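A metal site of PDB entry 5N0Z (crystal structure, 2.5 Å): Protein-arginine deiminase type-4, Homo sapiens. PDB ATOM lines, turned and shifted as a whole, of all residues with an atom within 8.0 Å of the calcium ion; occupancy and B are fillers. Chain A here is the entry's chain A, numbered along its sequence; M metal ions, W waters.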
ATOM      1  N   ASP A 357      19.785  -9.883  17.080  1.00  0.00           N
ATOM      2  CA  ASP A 357      19.280  -9.414  15.831  1.00  0.00           C
ATOM      3  C   ASP A 357      17.914  -9.910  15.465  1.00  0.00           C
ATOM      4  O   ASP A 357      17.237  -9.231  14.713  1.00  0.00           O
ATOM      5  CB  ASP A 357      20.270  -9.744  14.722  1.00  0.00           C
ATOM      6  CG  ASP A 357      21.576  -8.993  14.867  1.00  0.00           C
ATOM      7  OD1 ASP A 357      21.621  -7.969  15.608  1.00  0.00           O
ATOM      8  OD2 ASP A 357      22.562  -9.442  14.221  1.00  0.00           O
ATOM      9  N   GLU A 358      17.492 -11.070  15.938  1.00  0.00           N
ATOM     10  CA  GLU A 358      16.240 -11.618  15.446  1.00  0.00           C
ATOM     11  C   GLU A 358      15.094 -11.026  16.251  1.00  0.00           C
ATOM     12  O   GLU A 358      13.952 -11.055  15.766  1.00  0.00           O
ATOM     13  CB  GLU A 358      16.193 -13.156  15.461  1.00  0.00           C
ATOM     14  CG  GLU A 358      15.011 -13.832  14.687  1.00  0.00           C
ATOM     15  CD  GLU A 358      15.147 -13.893  13.155  1.00  0.00           C
ATOM     16  OE1 GLU A 358      14.107 -14.084  12.457  1.00  0.00           O
ATOM     17  OE2 GLU A 358      16.278 -13.775  12.596  1.00  0.00           O
ATOM     18  N   MET A 359      15.337 -10.468  17.442  1.00  0.00           N
ATOM     19  CA  MET A 359      14.201 -10.071  18.275  1.00  0.00           C
ATOM     20  C   MET A 359      14.436  -8.884  19.190  1.00  0.00           C
ATOM     21  O   MET A 359      15.582  -8.550  19.487  1.00  0.00           O
ATOM     22  CB  MET A 359      13.780 -11.294  19.083  1.00  0.00           C
ATOM     23  CG  MET A 359      14.357 -11.326  20.480  1.00  0.00           C
ATOM     24  SD  MET A 359      14.183 -12.959  21.195  1.00  0.00           S
ATOM     25  CE  MET A 359      15.024 -12.651  22.745  1.00  0.00           C
ATOM     26  N   PHE A 375       9.067  -8.323  19.966  1.00  0.00           N
ATOM     27  CA  PHE A 375       8.966  -7.902  18.612  1.00  0.00           C
ATOM     28  C   PHE A 375       9.988  -8.765  17.834  1.00  0.00           C
ATOM     29  O   PHE A 375      11.166  -8.775  18.133  1.00  0.00           O
ATOM     30  CB  PHE A 375       9.197  -6.401  18.529  1.00  0.00           C
ATOM     31  CG  PHE A 375       8.994  -5.818  17.172  1.00  0.00           C
ATOM     32  CD1 PHE A 375       8.240  -6.481  16.190  1.00  0.00           C
ATOM     33  CD2 PHE A 375       9.499  -4.569  16.886  1.00  0.00           C
ATOM     34  CE1 PHE A 375       8.060  -5.917  14.947  1.00  0.00           C
ATOM     35  CE2 PHE A 375       9.297  -4.004  15.643  1.00  0.00           C
ATOM     36  CZ  PHE A 375       8.586  -4.690  14.673  1.00  0.00           C
ATOM     37  N   ASP A 376       9.491  -9.485  16.853  1.00  0.00           N
ATOM     38  CA  ASP A 376      10.237 -10.506  16.157  1.00  0.00           C
ATOM     39  C   ASP A 376      10.497 -10.011  14.772  1.00  0.00           C
ATOM     40  O   ASP A 376       9.592  -9.827  13.972  1.00  0.00           O
ATOM     41  CB  ASP A 376       9.416 -11.805  16.152  1.00  0.00           C
ATOM     42  CG  ASP A 376      10.042 -12.918  15.289  1.00  0.00           C
ATOM     43  OD1 ASP A 376      11.201 -12.795  14.848  1.00  0.00           O
ATOM     44  OD2 ASP A 376       9.324 -13.929  15.053  1.00  0.00           O
ATOM     45  N   SER A 377      11.771  -9.820  14.496  1.00  0.00           N
ATOM     46  CA  SER A 377      12.238  -9.201  13.270  1.00  0.00           C
ATOM     47  C   SER A 377      11.979 -10.145  12.101  1.00  0.00           C
ATOM     48  O   SER A 377      12.133 -11.356  12.237  1.00  0.00           O
ATOM     49  CB  SER A 377      13.749  -8.913  13.415  1.00  0.00           C
ATOM     50  OG  SER A 377      14.372  -8.513  12.212  1.00  0.00           O
ATOM     51  N   PRO A 378      11.666  -9.603  10.932  1.00  0.00           N
ATOM     52  CA  PRO A 378      11.556 -10.431   9.748  1.00  0.00           C
ATOM     53  C   PRO A 378      12.914 -10.902   9.183  1.00  0.00           C
ATOM     54  O   PRO A 378      12.941 -11.474   8.096  1.00  0.00           O
ATOM     55  CB  PRO A 378      10.901  -9.467   8.753  1.00  0.00           C
ATOM     56  CG  PRO A 378      11.547  -8.157   9.086  1.00  0.00           C
ATOM     57  CD  PRO A 378      11.692  -8.163  10.585  1.00  0.00           C
ATOM     58  N   ARG A 379      14.003 -10.609   9.883  1.00  0.00           N
ATOM     59  CA  ARG A 379      15.337 -11.103   9.545  1.00  0.00           C
ATOM     60  C   ARG A 379      15.266 -12.552   9.087  1.00  0.00           C
ATOM     61  O   ARG A 379      15.719 -12.868   7.986  1.00  0.00           O
ATOM     62  CB  ARG A 379      16.272 -10.926  10.754  1.00  0.00           C
ATOM     63  CG  ARG A 379      17.740 -11.287  10.566  1.00  0.00           C
ATOM     64  CD  ARG A 379      18.445 -11.077  11.895  1.00  0.00           C
ATOM     65  NE  ARG A 379      19.766 -11.743  12.051  1.00  0.00           N
ATOM     66  CZ  ARG A 379      20.003 -12.852  12.761  1.00  0.00           C
ATOM     67  NH1 ARG A 379      21.241 -13.316  12.836  1.00  0.00           N
ATOM     68  NH2 ARG A 379      19.050 -13.521  13.391  1.00  0.00           N
ATOM     69  N   ASN A 380      14.649 -13.411   9.904  1.00  0.00           N
ATOM     70  CA  ASN A 380      14.346 -14.816   9.506  1.00  0.00           C
ATOM     71  C   ASN A 380      15.575 -15.660   9.056  1.00  0.00           C
ATOM     72  O   ASN A 380      15.546 -16.349   8.031  1.00  0.00           O
ATOM     73  CB  ASN A 380      13.215 -14.845   8.451  1.00  0.00           C
ATOM     74  CG  ASN A 380      11.861 -14.388   9.017  1.00  0.00           C
ATOM     75  OD1 ASN A 380      11.712 -14.200  10.232  1.00  0.00           O
ATOM     76  ND2 ASN A 380      10.867 -14.225   8.135  1.00  0.00           N
ATOM     77  N   ARG A 381      16.648 -15.596   9.841  1.00  0.00           N
ATOM     78  CA  ARG A 381      17.780 -16.510   9.691  1.00  0.00           C
ATOM     79  C   ARG A 381      17.581 -17.702  10.628  1.00  0.00           C
ATOM     80  O   ARG A 381      16.448 -17.980  11.050  1.00  0.00           O
ATOM     81  CB  ARG A 381      19.087 -15.770   9.956  1.00  0.00           C
ATOM     82  CG  ARG A 381      19.328 -14.694   8.923  1.00  0.00           C
ATOM     83  CD  ARG A 381      20.797 -14.370   8.749  1.00  0.00           C
ATOM     84  NE  ARG A 381      20.977 -13.658   7.497  1.00  0.00           N
ATOM     85  CZ  ARG A 381      22.157 -13.453   6.897  1.00  0.00           C
ATOM     86  NH1 ARG A 381      22.185 -12.790   5.735  1.00  0.00           N
ATOM     87  NH2 ARG A 381      23.294 -13.880   7.439  1.00  0.00           N
ATOM     88  N   LEU A 383      17.619 -18.271  13.711  1.00  0.00           N
ATOM     89  CA  LEU A 383      16.899 -18.122  14.982  1.00  0.00           C
ATOM     90  C   LEU A 383      15.402 -17.974  14.757  1.00  0.00           C
ATOM     91  O   LEU A 383      14.668 -17.824  15.734  1.00  0.00           O
ATOM     92  CB  LEU A 383      17.415 -16.938  15.788  1.00  0.00           C
ATOM     93  CG  LEU A 383      18.684 -17.223  16.577  1.00  0.00           C
ATOM     94  CD1 LEU A 383      19.482 -15.959  16.870  1.00  0.00           C
ATOM     95  CD2 LEU A 383      18.336 -17.968  17.856  1.00  0.00           C
ATOM     96  N   LYS A 384      14.988 -18.046  13.493  1.00  0.00           N
ATOM     97  CA  LYS A 384      13.619 -17.779  13.035  1.00  0.00           C
ATOM     98  C   LYS A 384      12.490 -18.261  13.973  1.00  0.00           C
ATOM     99  O   LYS A 384      11.464 -17.581  14.118  1.00  0.00           O
ATOM    100  CB  LYS A 384      13.431 -18.350  11.613  1.00  0.00           C
ATOM    101  CG  LYS A 384      12.004 -18.455  11.129  1.00  0.00           C
ATOM    102  CD  LYS A 384      11.933 -18.927   9.680  1.00  0.00           C
ATOM    103  CE  LYS A 384      10.506 -19.373   9.335  1.00  0.00           C
ATOM    104  NZ  LYS A 384      10.108 -18.980   7.957  1.00  0.00           N
ATOM    105  N   GLU A 385      12.677 -19.424  14.593  1.00  0.00           N
ATOM    106  CA  GLU A 385      11.662 -20.053  15.423  1.00  0.00           C
ATOM    107  C   GLU A 385      11.766 -19.652  16.878  1.00  0.00           C
ATOM    108  O   GLU A 385      10.767 -19.800  17.607  1.00  0.00           O
ATOM    109  CB  GLU A 385      11.766 -21.580  15.316  1.00  0.00           C
ATOM    110  CG  GLU A 385      11.449 -22.114  13.929  1.00  0.00           C
ATOM    111  CD  GLU A 385      10.049 -21.738  13.468  1.00  0.00           C
ATOM    112  OE1 GLU A 385       9.918 -21.216  12.334  1.00  0.00           O
ATOM    113  OE2 GLU A 385       9.108 -21.948  14.284  1.00  0.00           O
ATOM    114  N   PHE A 386      12.946 -19.179  17.289  1.00  0.00           N
ATOM    115  CA  PHE A 386      13.212 -18.888  18.714  1.00  0.00           C
ATOM    116  C   PHE A 386      12.163 -17.970  19.367  1.00  0.00           C
ATOM    117  O   PHE A 386      11.712 -18.271  20.482  1.00  0.00           O
ATOM    118  CB  PHE A 386      14.641 -18.333  18.964  1.00  0.00           C
ATOM    119  CG  PHE A 386      14.943 -18.118  20.431  1.00  0.00           C
ATOM    120  CD1 PHE A 386      15.042 -19.211  21.294  1.00  0.00           C
ATOM    121  CD2 PHE A 386      15.054 -16.846  20.958  1.00  0.00           C
ATOM    122  CE1 PHE A 386      15.274 -19.026  22.660  1.00  0.00           C
ATOM    123  CE2 PHE A 386      15.296 -16.659  22.321  1.00  0.00           C
ATOM    124  CZ  PHE A 386      15.399 -17.744  23.173  1.00  0.00           C
ATOM    125  N   PRO A 387      11.774 -16.860  18.689  1.00  0.00           N
ATOM    126  CA  PRO A 387      10.753 -15.973  19.270  1.00  0.00           C
ATOM    127  C   PRO A 387       9.368 -16.636  19.378  1.00  0.00           C
ATOM    128  O   PRO A 387       8.678 -16.480  20.393  1.00  0.00           O
ATOM    129  CB  PRO A 387      10.747 -14.783  18.308  1.00  0.00           C
ATOM    130  CG  PRO A 387      12.068 -14.812  17.641  1.00  0.00           C
ATOM    131  CD  PRO A 387      12.298 -16.276  17.442  1.00  0.00           C
ATOM    132  N   ILE A 388       8.995 -17.418  18.359  1.00  0.00           N
ATOM    133  CA  ILE A 388       7.706 -18.085  18.363  1.00  0.00           C
ATOM    134  C   ILE A 388       7.707 -19.207  19.430  1.00  0.00           C
ATOM    135  O   ILE A 388       6.879 -19.219  20.351  1.00  0.00           O
ATOM    136  CB  ILE A 388       7.372 -18.705  16.984  1.00  0.00           C
ATOM    137  CG1 ILE A 388       7.485 -17.662  15.868  1.00  0.00           C
ATOM    138  CG2 ILE A 388       5.964 -19.311  17.009  1.00  0.00           C
ATOM    139  CD1 ILE A 388       7.528 -18.246  14.472  1.00  0.00           C
ATOM    140  N   TYR A 398       3.667 -11.798  21.510  1.00  0.00           N
ATOM    141  CA  TYR A 398       4.378 -11.778  20.289  1.00  0.00           C
ATOM    142  C   TYR A 398       3.792 -10.763  19.311  1.00  0.00           C
ATOM    143  O   TYR A 398       2.580 -10.534  19.279  1.00  0.00           O
ATOM    144  CB  TYR A 398       4.246 -13.152  19.744  1.00  0.00           C
ATOM    145  CG  TYR A 398       4.947 -13.336  18.454  1.00  0.00           C
ATOM    146  CD1 TYR A 398       4.275 -13.106  17.225  1.00  0.00           C
ATOM    147  CD2 TYR A 398       6.261 -13.766  18.427  1.00  0.00           C
ATOM    148  CE1 TYR A 398       4.933 -13.307  16.017  1.00  0.00           C
ATOM    149  CE2 TYR A 398       6.906 -13.956  17.222  1.00  0.00           C
ATOM    150  CZ  TYR A 398       6.250 -13.735  16.034  1.00  0.00           C
ATOM    151  OH  TYR A 398       6.957 -13.898  14.873  1.00  0.00           O
ATOM    152  N   VAL A 399       4.681 -10.148  18.514  1.00  0.00           N
ATOM    153  CA  VAL A 399       4.335  -9.305  17.363  1.00  0.00           C
ATOM    154  C   VAL A 399       5.370  -9.481  16.289  1.00  0.00           C
ATOM    155  O   VAL A 399       6.540  -9.670  16.612  1.00  0.00           O
ATOM    156  CB  VAL A 399       4.458  -7.795  17.641  1.00  0.00           C
ATOM    157  CG1 VAL A 399       3.474  -7.025  16.772  1.00  0.00           C
ATOM    158  CG2 VAL A 399       4.250  -7.463  19.088  1.00  0.00           C
ATOM    159  N   THR A 400       4.970  -9.313  15.036  1.00  0.00           N
ATOM    160  CA  THR A 400       5.944  -9.250  13.944  1.00  0.00           C
ATOM    161  C   THR A 400       5.498  -8.318  12.799  1.00  0.00           C
ATOM    162  O   THR A 400       4.323  -8.054  12.587  1.00  0.00           O
ATOM    163  CB  THR A 400       6.243 -10.668  13.413  1.00  0.00           C
ATOM    164  OG1 THR A 400       7.495 -10.652  12.710  1.00  0.00           O
ATOM    165  CG2 THR A 400       5.122 -11.177  12.473  1.00  0.00           C
ATOM    166  N   ARG A 401       6.479  -7.837  12.034  1.00  0.00           N
ATOM    167  CA  ARG A 401       6.219  -6.924  10.938  1.00  0.00           C
ATOM    168  C   ARG A 401       7.151  -7.082   9.737  1.00  0.00           C
ATOM    169  O   ARG A 401       8.252  -7.607   9.839  1.00  0.00           O
ATOM    170  CB  ARG A 401       6.300  -5.483  11.483  1.00  0.00           C
ATOM    171  CG  ARG A 401       5.082  -5.023  12.259  1.00  0.00           C
ATOM    172  CD  ARG A 401       3.838  -5.168  11.417  1.00  0.00           C
ATOM    173  NE  ARG A 401       2.691  -4.595  12.076  1.00  0.00           N
ATOM    174  CZ  ARG A 401       1.975  -5.163  13.030  1.00  0.00           C
ATOM    175  NH1 ARG A 401       2.272  -6.373  13.487  1.00  0.00           N
ATOM    176  NH2 ARG A 401       0.943  -4.496  13.529  1.00  0.00           N
ATOM    177  N   PRO A 403       7.933  -8.059   5.492  1.00  0.00           N
ATOM    178  CA  PRO A 403       7.787  -9.275   4.716  1.00  0.00           C
ATOM    179  C   PRO A 403       8.659 -10.389   5.267  1.00  0.00           C
ATOM    180  O   PRO A 403       9.831 -10.164   5.614  1.00  0.00           O
ATOM    181  CB  PRO A 403       8.220  -8.848   3.300  1.00  0.00           C
ATOM    182  CG  PRO A 403       9.192  -7.741   3.528  1.00  0.00           C
ATOM    183  CD  PRO A 403       8.802  -7.070   4.812  1.00  0.00           C
ATOM    184  N   GLN A 404       8.059 -11.577   5.359  1.00  0.00           N
ATOM    185  CA  GLN A 404       8.671 -12.734   6.010  1.00  0.00           C
ATOM    186  C   GLN A 404       9.580 -13.539   5.074  1.00  0.00           C
ATOM    187  O   GLN A 404      10.460 -14.263   5.553  1.00  0.00           O
ATOM    188  CB  GLN A 404       7.571 -13.599   6.658  1.00  0.00           C
ATOM    189  CG  GLN A 404       6.798 -12.867   7.770  1.00  0.00           C
ATOM    190  CD  GLN A 404       7.698 -12.363   8.920  1.00  0.00           C
ATOM    191  OE1 GLN A 404       8.607 -13.065   9.372  1.00  0.00           O
ATOM    192  NE2 GLN A 404       7.437 -11.135   9.381  1.00  0.00           N
ATOM    193  N   PHE A 414      17.671  -6.373  14.700  1.00  0.00           N
ATOM    194  CA  PHE A 414      17.339  -5.556  15.859  1.00  0.00           C
ATOM    195  C   PHE A 414      18.513  -5.146  16.682  1.00  0.00           C
ATOM    196  O   PHE A 414      18.344  -4.492  17.706  1.00  0.00           O
ATOM    197  CB  PHE A 414      16.229  -6.236  16.628  1.00  0.00           C
ATOM    198  CG  PHE A 414      14.895  -6.159  15.929  1.00  0.00           C
ATOM    199  CD1 PHE A 414      14.771  -5.611  14.612  1.00  0.00           C
ATOM    200  CD2 PHE A 414      13.735  -6.614  16.575  1.00  0.00           C
ATOM    201  CE1 PHE A 414      13.557  -5.503  13.999  1.00  0.00           C
ATOM    202  CE2 PHE A 414      12.508  -6.511  15.952  1.00  0.00           C
ATOM    203  CZ  PHE A 414      12.418  -5.966  14.669  1.00  0.00           C
HETATM  204 CA    CA M   1      11.621 -13.632  12.494  1.00  0.00          CA
HETATM  205  O   HOH W   1       9.515 -12.716  12.074  1.00  0.00           O
HETATM  206  O   HOH W   2      10.740 -15.552  12.956  1.00  0.00           O
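The side-chain amide nitrogen (ND2) of Asn 380 lies close to the backbone carbonyl oxygen (O) of Pro 378 (3.4 Å). O of Gln 404 lies within hydrogen-bond range of ND2 of Asn 380 (2.6 Å). OG of Ser 377 sits close to N of Arg 379, 3.2 Å away. The guanidinium group (NH2) of Arg 379 is in salt-bridge range of the side-chain carboxylate (OE2) of Glu 358, at 2.9 Å. The side-chain carboxylate of Glu 358 lies within hydrogen-bond range of the backbone NH of Arg 381. The backbone carbonyl oxygen (O) of Asp 376 lies within hydrogen-bond range of the side-chain hydroxyl (OG1) of Thr 400 (2.6 Å). N of Asp 376 is in hydrogen-bond range of O of Val 399, at 3.0 Å.
Four residues have an atom within 4 Å of the calcium ion: Glu 358, Asp 376, Ser 377 and Asn 380.
The calcium ion is bound by water W2, OD1 of Asn 380, water W1, O of Ser 377, OE1 of Glu 358 and OD1 of Asp 376.
Water W2 lies within hydrogen-bond range of the backbone carbonyl oxygen of Lys 384 (2.4 Å) and the side-chain carboxylate of Asp 376 (3.0 Å). Water W1 lies within hydrogen-bond range of the side-chain amide oxygen of Gln 404 (2.9 Å), the side-chain hydroxyl of Thr 400 (3.0 Å) and the side-chain carboxylate of Asp 376 (3.2 Å).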
